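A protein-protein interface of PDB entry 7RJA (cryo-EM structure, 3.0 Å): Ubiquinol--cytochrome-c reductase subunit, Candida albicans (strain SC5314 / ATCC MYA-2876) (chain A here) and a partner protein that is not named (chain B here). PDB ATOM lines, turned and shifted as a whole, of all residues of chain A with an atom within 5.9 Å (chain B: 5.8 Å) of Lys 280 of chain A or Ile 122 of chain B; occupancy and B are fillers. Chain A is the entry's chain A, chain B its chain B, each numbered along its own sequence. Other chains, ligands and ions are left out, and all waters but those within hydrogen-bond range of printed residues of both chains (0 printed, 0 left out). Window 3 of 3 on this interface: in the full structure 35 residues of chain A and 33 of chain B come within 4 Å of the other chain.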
ATOM      1  N   PHE A 272     -35.083  13.727 -22.457  1.00  0.00           N
ATOM      2  CA  PHE A 272     -33.776  13.358 -21.934  1.00  0.00           C
ATOM      3  C   PHE A 272     -33.356  12.001 -22.471  1.00  0.00           C
ATOM      4  O   PHE A 272     -34.133  11.045 -22.420  1.00  0.00           O
ATOM      5  CB  PHE A 272     -33.805  13.335 -20.410  1.00  0.00           C
ATOM      6  CG  PHE A 272     -32.547  12.811 -19.784  1.00  0.00           C
ATOM      7  CD1 PHE A 272     -31.429  13.611 -19.675  1.00  0.00           C
ATOM      8  CD2 PHE A 272     -32.488  11.524 -19.293  1.00  0.00           C
ATOM      9  CE1 PHE A 272     -30.280  13.134 -19.098  1.00  0.00           C
ATOM     10  CE2 PHE A 272     -31.340  11.045 -18.713  1.00  0.00           C
ATOM     11  CZ  PHE A 272     -30.236  11.850 -18.616  1.00  0.00           C
ATOM     12  N   LEU A 274     -29.955   9.522 -21.977  1.00  0.00           N
ATOM     13  CA  LEU A 274     -28.762   9.485 -21.140  1.00  0.00           C
ATOM     14  C   LEU A 274     -27.493   9.551 -21.976  1.00  0.00           C
ATOM     15  O   LEU A 274     -26.540  10.249 -21.615  1.00  0.00           O
ATOM     16  CB  LEU A 274     -28.762   8.221 -20.283  1.00  0.00           C
ATOM     17  CG  LEU A 274     -27.502   7.976 -19.452  1.00  0.00           C
ATOM     18  CD1 LEU A 274     -27.302   9.099 -18.456  1.00  0.00           C
ATOM     19  CD2 LEU A 274     -27.588   6.642 -18.739  1.00  0.00           C
ATOM     20  N   HIS A 275     -27.459   8.830 -23.091  1.00  0.00           N
ATOM     21  CA  HIS A 275     -26.257   8.742 -23.905  1.00  0.00           C
ATOM     22  C   HIS A 275     -26.090   9.909 -24.866  1.00  0.00           C
ATOM     23  O   HIS A 275     -25.043  10.007 -25.510  1.00  0.00           O
ATOM     24  CB  HIS A 275     -26.256   7.431 -24.688  1.00  0.00           C
ATOM     25  CG  HIS A 275     -26.288   6.218 -23.814  1.00  0.00           C
ATOM     26  ND1 HIS A 275     -27.441   5.505 -23.570  1.00  0.00           N
ATOM     27  CD2 HIS A 275     -25.308   5.600 -23.113  1.00  0.00           C
ATOM     28  CE1 HIS A 275     -27.170   4.495 -22.764  1.00  0.00           C
ATOM     29  NE2 HIS A 275     -25.882   4.530 -22.471  1.00  0.00           N
ATOM     30  N   SER A 276     -27.075  10.792 -24.978  1.00  0.00           N
ATOM     31  CA  SER A 276     -26.908  11.974 -25.810  1.00  0.00           C
ATOM     32  C   SER A 276     -25.836  12.880 -25.221  1.00  0.00           C
ATOM     33  O   SER A 276     -25.598  12.893 -24.012  1.00  0.00           O
ATOM     34  CB  SER A 276     -28.227  12.731 -25.932  1.00  0.00           C
ATOM     35  OG  SER A 276     -28.072  13.884 -26.736  1.00  0.00           O
ATOM     36  N   THR A 277     -25.172  13.640 -26.093  1.00  0.00           N
ATOM     37  CA  THR A 277     -24.086  14.500 -25.636  1.00  0.00           C
ATOM     38  C   THR A 277     -24.588  15.553 -24.658  1.00  0.00           C
ATOM     39  O   THR A 277     -23.943  15.820 -23.638  1.00  0.00           O
ATOM     40  CB  THR A 277     -23.405  15.170 -26.827  1.00  0.00           C
ATOM     41  OG1 THR A 277     -24.362  15.951 -27.549  1.00  0.00           O
ATOM     42  CG2 THR A 277     -22.807  14.131 -27.749  1.00  0.00           C
ATOM     43  N   ILE A 278     -25.742  16.161 -24.949  1.00  0.00           N
ATOM     44  CA  ILE A 278     -26.289  17.204 -24.083  1.00  0.00           C
ATOM     45  C   ILE A 278     -26.884  16.659 -22.799  1.00  0.00           C
ATOM     46  O   ILE A 278     -27.388  17.442 -21.985  1.00  0.00           O
ATOM     47  CB  ILE A 278     -27.373  18.021 -24.813  1.00  0.00           C
ATOM     48  CG1 ILE A 278     -28.571  17.138 -25.155  1.00  0.00           C
ATOM     49  CG2 ILE A 278     -26.802  18.642 -26.067  1.00  0.00           C
ATOM     50  CD1 ILE A 278     -29.661  17.862 -25.903  1.00  0.00           C
ATOM     51  N   ALA A 279     -26.838  15.344 -22.583  1.00  0.00           N
ATOM     52  CA  ALA A 279     -27.438  14.774 -21.384  1.00  0.00           C
ATOM     53  C   ALA A 279     -26.918  15.445 -20.124  1.00  0.00           C
ATOM     54  O   ALA A 279     -27.663  15.606 -19.153  1.00  0.00           O
ATOM     55  CB  ALA A 279     -27.164  13.272 -21.326  1.00  0.00           C
ATOM     56  N   LYS A 280     -25.654  15.851 -20.121  1.00  0.00           N
ATOM     57  CA  LYS A 280     -25.060  16.504 -18.964  1.00  0.00           C
ATOM     58  C   LYS A 280     -25.328  18.001 -18.925  1.00  0.00           C
ATOM     59  O   LYS A 280     -24.871  18.667 -17.990  1.00  0.00           O
ATOM     60  CB  LYS A 280     -23.551  16.262 -18.950  1.00  0.00           C
ATOM     61  CG  LYS A 280     -23.165  14.828 -18.668  1.00  0.00           C
ATOM     62  CD  LYS A 280     -21.662  14.675 -18.574  1.00  0.00           C
ATOM     63  CE  LYS A 280     -21.270  13.229 -18.353  1.00  0.00           C
ATOM     64  NZ  LYS A 280     -21.694  12.748 -17.013  1.00  0.00           N
ATOM     65  N   PHE A 281     -26.047  18.549 -19.906  1.00  0.00           N
ATOM     66  CA  PHE A 281     -26.248  19.986 -19.997  1.00  0.00           C
ATOM     67  C   PHE A 281     -27.699  20.399 -20.199  1.00  0.00           C
ATOM     68  O   PHE A 281     -27.982  21.599 -20.194  1.00  0.00           O
ATOM     69  CB  PHE A 281     -25.404  20.559 -21.142  1.00  0.00           C
ATOM     70  CG  PHE A 281     -24.028  19.974 -21.223  1.00  0.00           C
ATOM     71  CD1 PHE A 281     -23.154  20.083 -20.161  1.00  0.00           C
ATOM     72  CD2 PHE A 281     -23.611  19.306 -22.356  1.00  0.00           C
ATOM     73  CE1 PHE A 281     -21.892  19.544 -20.232  1.00  0.00           C
ATOM     74  CE2 PHE A 281     -22.351  18.766 -22.428  1.00  0.00           C
ATOM     75  CZ  PHE A 281     -21.491  18.886 -21.365  1.00  0.00           C
ATOM     76  N   THR A 282     -28.621  19.456 -20.370  1.00  0.00           N
ATOM     77  CA  THR A 282     -30.016  19.822 -20.564  1.00  0.00           C
ATOM     78  C   THR A 282     -30.532  20.606 -19.364  1.00  0.00           C
ATOM     79  O   THR A 282     -30.200  20.309 -18.215  1.00  0.00           O
ATOM     80  CB  THR A 282     -30.872  18.576 -20.783  1.00  0.00           C
ATOM     81  OG1 THR A 282     -30.590  17.612 -19.763  1.00  0.00           O
ATOM     82  CG2 THR A 282     -30.604  17.971 -22.145  1.00  0.00           C
ATOM     83  N   GLN A 291     -29.109  11.947 -13.392  1.00  0.00           N
ATOM     84  CA  GLN A 291     -27.765  11.626 -13.848  1.00  0.00           C
ATOM     85  C   GLN A 291     -26.779  11.439 -12.707  1.00  0.00           C
ATOM     86  O   GLN A 291     -25.630  11.067 -12.958  1.00  0.00           O
ATOM     87  CB  GLN A 291     -27.246  12.719 -14.779  1.00  0.00           C
ATOM     88  CG  GLN A 291     -27.815  12.657 -16.170  1.00  0.00           C
ATOM     89  CD  GLN A 291     -27.283  13.759 -17.049  1.00  0.00           C
ATOM     90  OE1 GLN A 291     -26.451  13.524 -17.923  1.00  0.00           O
ATOM     91  NE2 GLN A 291     -27.751  14.977 -16.816  1.00  0.00           N
ATOM     92  N   LYS B  53     -19.171  14.604 -32.490  1.00  0.00           N
ATOM     93  CA  LYS B  53     -19.525  14.578 -31.078  1.00  0.00           C
ATOM     94  C   LYS B  53     -18.840  15.683 -30.283  1.00  0.00           C
ATOM     95  O   LYS B  53     -19.335  16.052 -29.215  1.00  0.00           O
ATOM     96  CB  LYS B  53     -19.184  13.216 -30.478  1.00  0.00           C
ATOM     97  CG  LYS B  53     -20.091  12.108 -30.971  1.00  0.00           C
ATOM     98  CD  LYS B  53     -21.415  12.108 -30.242  1.00  0.00           C
ATOM     99  CE  LYS B  53     -22.415  11.160 -30.887  1.00  0.00           C
ATOM    100  NZ  LYS B  53     -22.700  11.501 -32.304  1.00  0.00           N
ATOM    101  N   LEU B  57     -19.585  21.139 -27.764  1.00  0.00           N
ATOM    102  CA  LEU B  57     -19.349  20.987 -26.328  1.00  0.00           C
ATOM    103  C   LEU B  57     -18.664  22.209 -25.717  1.00  0.00           C
ATOM    104  O   LEU B  57     -19.286  22.965 -24.967  1.00  0.00           O
ATOM    105  CB  LEU B  57     -18.540  19.714 -26.072  1.00  0.00           C
ATOM    106  CG  LEU B  57     -19.411  18.463 -25.958  1.00  0.00           C
ATOM    107  CD1 LEU B  57     -20.051  18.145 -27.287  1.00  0.00           C
ATOM    108  CD2 LEU B  57     -18.596  17.289 -25.471  1.00  0.00           C
ATOM    109  N   LEU B  65     -22.109  23.527 -20.929  1.00  0.00           N
ATOM    110  CA  LEU B  65     -23.189  23.748 -19.982  1.00  0.00           C
ATOM    111  C   LEU B  65     -23.748  25.157 -20.072  1.00  0.00           C
ATOM    112  O   LEU B  65     -24.865  25.393 -19.605  1.00  0.00           O
ATOM    113  CB  LEU B  65     -22.693  23.442 -18.570  1.00  0.00           C
ATOM    114  CG  LEU B  65     -23.720  23.441 -17.442  1.00  0.00           C
ATOM    115  CD1 LEU B  65     -23.247  22.518 -16.343  1.00  0.00           C
ATOM    116  CD2 LEU B  65     -23.917  24.828 -16.866  1.00  0.00           C
ATOM    117  N   ARG B  69     -27.552  25.507 -22.206  1.00  0.00           N
ATOM    118  CA  ARG B  69     -28.579  26.161 -21.403  1.00  0.00           C
ATOM    119  C   ARG B  69     -29.129  27.388 -22.116  1.00  0.00           C
ATOM    120  O   ARG B  69     -30.348  27.590 -22.177  1.00  0.00           O
ATOM    121  CB  ARG B  69     -28.006  26.547 -20.044  1.00  0.00           C
ATOM    122  CG  ARG B  69     -27.699  25.370 -19.141  1.00  0.00           C
ATOM    123  CD  ARG B  69     -28.959  24.719 -18.626  1.00  0.00           C
ATOM    124  NE  ARG B  69     -28.869  24.440 -17.199  1.00  0.00           N
ATOM    125  CZ  ARG B  69     -28.293  23.367 -16.679  1.00  0.00           C
ATOM    126  NH1 ARG B  69     -27.742  22.440 -17.442  1.00  0.00           N
ATOM    127  NH2 ARG B  69     -28.269  23.220 -15.359  1.00  0.00           N
ATOM    128  N   HIS B 117     -11.092  15.378 -20.956  1.00  0.00           N
ATOM    129  CA  HIS B 117     -12.183  14.926 -20.109  1.00  0.00           C
ATOM    130  C   HIS B 117     -13.494  14.822 -20.867  1.00  0.00           C
ATOM    131  O   HIS B 117     -14.360  14.033 -20.479  1.00  0.00           O
ATOM    132  CB  HIS B 117     -12.333  15.853 -18.913  1.00  0.00           C
ATOM    133  CG  HIS B 117     -12.816  17.227 -19.255  1.00  0.00           C
ATOM    134  ND1 HIS B 117     -14.148  17.524 -19.443  1.00  0.00           N
ATOM    135  CD2 HIS B 117     -12.145  18.390 -19.420  1.00  0.00           C
ATOM    136  CE1 HIS B 117     -14.276  18.809 -19.719  1.00  0.00           C
ATOM    137  NE2 HIS B 117     -13.076  19.358 -19.711  1.00  0.00           N
ATOM    138  N   GLU B 118     -13.664  15.600 -21.934  1.00  0.00           N
ATOM    139  CA  GLU B 118     -14.803  15.392 -22.813  1.00  0.00           C
ATOM    140  C   GLU B 118     -14.595  14.191 -23.718  1.00  0.00           C
ATOM    141  O   GLU B 118     -15.555  13.480 -24.029  1.00  0.00           O
ATOM    142  CB  GLU B 118     -15.051  16.637 -23.652  1.00  0.00           C
ATOM    143  CG  GLU B 118     -15.980  17.618 -22.992  1.00  0.00           C
ATOM    144  CD  GLU B 118     -15.716  19.038 -23.417  1.00  0.00           C
ATOM    145  OE1 GLU B 118     -14.923  19.248 -24.358  1.00  0.00           O
ATOM    146  OE2 GLU B 118     -16.304  19.949 -22.803  1.00  0.00           O
ATOM    147  N   PHE B 119     -13.357  13.947 -24.144  1.00  0.00           N
ATOM    148  CA  PHE B 119     -13.094  12.792 -24.988  1.00  0.00           C
ATOM    149  C   PHE B 119     -13.359  11.492 -24.249  1.00  0.00           C
ATOM    150  O   PHE B 119     -13.683  10.481 -24.878  1.00  0.00           O
ATOM    151  CB  PHE B 119     -11.653  12.819 -25.482  1.00  0.00           C
ATOM    152  CG  PHE B 119     -11.339  11.745 -26.477  1.00  0.00           C
ATOM    153  CD1 PHE B 119     -12.014  11.682 -27.679  1.00  0.00           C
ATOM    154  CD2 PHE B 119     -10.379  10.794 -26.207  1.00  0.00           C
ATOM    155  CE1 PHE B 119     -11.729  10.698 -28.592  1.00  0.00           C
ATOM    156  CE2 PHE B 119     -10.092   9.806 -27.119  1.00  0.00           C
ATOM    157  CZ  PHE B 119     -10.770   9.759 -28.311  1.00  0.00           C
ATOM    158  N   ASN B 120     -13.220  11.493 -22.926  1.00  0.00           N
ATOM    159  CA  ASN B 120     -13.385  10.270 -22.154  1.00  0.00           C
ATOM    160  C   ASN B 120     -14.738  10.157 -21.468  1.00  0.00           C
ATOM    161  O   ASN B 120     -15.166   9.038 -21.171  1.00  0.00           O
ATOM    162  CB  ASN B 120     -12.281  10.161 -21.098  1.00  0.00           C
ATOM    163  CG  ASN B 120     -10.944   9.792 -21.697  1.00  0.00           C
ATOM    164  OD1 ASN B 120     -10.690   8.629 -22.004  1.00  0.00           O
ATOM    165  ND2 ASN B 120     -10.076  10.780 -21.865  1.00  0.00           N
ATOM    166  N   GLU B 121     -15.421  11.270 -21.213  1.00  0.00           N
ATOM    167  CA  GLU B 121     -16.681  11.243 -20.481  1.00  0.00           C
ATOM    168  C   GLU B 121     -17.903  11.437 -21.363  1.00  0.00           C
ATOM    169  O   GLU B 121     -18.943  10.829 -21.095  1.00  0.00           O
ATOM    170  CB  GLU B 121     -16.687  12.326 -19.400  1.00  0.00           C
ATOM    171  CG  GLU B 121     -15.632  12.141 -18.332  1.00  0.00           C
ATOM    172  CD  GLU B 121     -15.735  13.176 -17.233  1.00  0.00           C
ATOM    173  OE1 GLU B 121     -16.613  14.057 -17.330  1.00  0.00           O
ATOM    174  OE2 GLU B 121     -14.940  13.108 -16.274  1.00  0.00           O
ATOM    175  N   ILE B 122     -17.807  12.259 -22.404  1.00  0.00           N
ATOM    176  CA  ILE B 122     -18.968  12.645 -23.197  1.00  0.00           C
ATOM    177  C   ILE B 122     -18.894  12.166 -24.637  1.00  0.00           C
ATOM    178  O   ILE B 122     -19.948  12.014 -25.272  1.00  0.00           O
ATOM    179  CB  ILE B 122     -19.175  14.174 -23.169  1.00  0.00           C
ATOM    180  CG1 ILE B 122     -19.477  14.638 -21.748  1.00  0.00           C
ATOM    181  CG2 ILE B 122     -20.292  14.579 -24.109  1.00  0.00           C
ATOM    182  CD1 ILE B 122     -19.376  16.127 -21.562  1.00  0.00           C
ATOM    183  N   VAL B 123     -17.708  11.908 -25.174  1.00  0.00           N
ATOM    184  CA  VAL B 123     -17.532  11.600 -26.585  1.00  0.00           C
ATOM    185  C   VAL B 123     -17.417  10.100 -26.820  1.00  0.00           C
ATOM    186  O   VAL B 123     -18.250   9.508 -27.503  1.00  0.00           O
ATOM    187  CB  VAL B 123     -16.306  12.342 -27.158  1.00  0.00           C
ATOM    188  CG1 VAL B 123     -15.964  11.812 -28.535  1.00  0.00           C
ATOM    189  CG2 VAL B 123     -16.570  13.832 -27.198  1.00  0.00           C
ATOM    190  N   LEU B 124     -16.391   9.471 -26.266  1.00  0.00           N
ATOM    191  CA  LEU B 124     -16.203   8.047 -26.504  1.00  0.00           C
ATOM    192  C   LEU B 124     -17.391   7.245 -25.985  1.00  0.00           C
ATOM    193  O   LEU B 124     -17.887   6.364 -26.696  1.00  0.00           O
ATOM    194  CB  LEU B 124     -14.904   7.549 -25.872  1.00  0.00           C
ATOM    195  CG  LEU B 124     -13.632   7.896 -26.640  1.00  0.00           C
ATOM    196  CD1 LEU B 124     -12.417   7.429 -25.870  1.00  0.00           C
ATOM    197  CD2 LEU B 124     -13.654   7.274 -28.019  1.00  0.00           C
ATOM    198  N   PRO B 125     -17.874   7.492 -24.765  1.00  0.00           N
ATOM    199  CA  PRO B 125     -19.077   6.771 -24.326  1.00  0.00           C
ATOM    200  C   PRO B 125     -20.268   7.006 -25.233  1.00  0.00           C
ATOM    201  O   PRO B 125     -20.956   6.053 -25.619  1.00  0.00           O
ATOM    202  CB  PRO B 125     -19.315   7.323 -22.916  1.00  0.00           C
ATOM    203  CG  PRO B 125     -17.993   7.806 -22.475  1.00  0.00           C
ATOM    204  CD  PRO B 125     -17.347   8.358 -23.700  1.00  0.00           C
ATOM    205  N   THR B 126     -20.517   8.262 -25.603  1.00  0.00           N
ATOM    206  CA  THR B 126     -21.641   8.569 -26.479  1.00  0.00           C
ATOM    207  C   THR B 126     -21.450   7.965 -27.863  1.00  0.00           C
ATOM    208  O   THR B 126     -22.396   7.420 -28.443  1.00  0.00           O
ATOM    209  CB  THR B 126     -21.820  10.078 -26.587  1.00  0.00           C
ATOM    210  OG1 THR B 126     -22.118  10.618 -25.296  1.00  0.00           O
ATOM    211  CG2 THR B 126     -22.943  10.401 -27.540  1.00  0.00           C
ATOM    212  N   ALA B 127     -20.243   8.068 -28.420  1.00  0.00           N
ATOM    213  CA  ALA B 127     -20.001   7.508 -29.742  1.00  0.00           C
ATOM    214  C   ALA B 127     -20.187   6.000 -29.736  1.00  0.00           C
ATOM    215  O   ALA B 127     -20.792   5.436 -30.654  1.00  0.00           O
ATOM    216  CB  ALA B 127     -18.599   7.873 -30.218  1.00  0.00           C
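Of chain B, only Ile 122 (3.9 Å) comes within 4 Å of Lys 280 of chain A. Of chain A, only Thr 277 (3.9 Å), Lys 280 (3.9 Å) and Phe 281 (3.5 Å) come within 4 Å of Ile 122 of chain B. Printed residues of chain B within 4 Å of Thr 277 of chain A: Lys 53 (3.5 Å), Ile 122 (3.9 Å) and Thr 126 (3.7 Å). Printed residues of chain A within 4 Å of Lys 53 of chain B: Thr 277. Of the printed residues of chain B, Thr 282 of chain A touches Arg 69. Of the printed residues of chain A, Arg 69 of chain B touches Phe 281 (2.9 Å) and Thr 282 (3.3 Å). The nearest printed residue of chain B that does not touch His 275 of chain A is Pro 125 of chain B (5.0 Å).
N of Lys 280 of chain A is in hydrogen-bond range of OE1 of Gln 291 of chain A (3.3 Å). The backbone carbonyl oxygen of Ile 122 of chain B is in hydrogen-bond range of the side-chain hydroxyl of Thr 126 of chain B, 2.6 Å away.
Among the printed residues, pairs that only touch across the chains: Phe 281 of chain A with Ile 122 of chain B (3.5 Å), Thr 277 of chain A with Lys 53 of chain B (3.5 Å), Phe 281 of chain A with Leu 65 of chain B (3.7 Å), Thr 277 of chain A with Thr 126 of chain B (3.7 Å), Lys 280 of chain A with Ile 122 of chain B (3.9 Å) and Thr 277 of chain A with Ile 122 of chain B (3.9 Å).
O of His 275 of chain A sits close to OG1 of Thr 126 of chain B (3.0 Å). The backbone carbonyl oxygen (O) of Phe 281 of chain A is in hydrogen-bond range of the guanidinium group (NH1) of Arg 69 of chain B, at 2.9 Å. The backbone carbonyl oxygen (O) of Thr 282 of chain A sits at hydrogen-bond distance from the guanidinium group (NH1) of Arg 69 of chain B (3.3 Å).
Of the 15 printed residues of chain B, 5 touch a printed residue of chain A.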
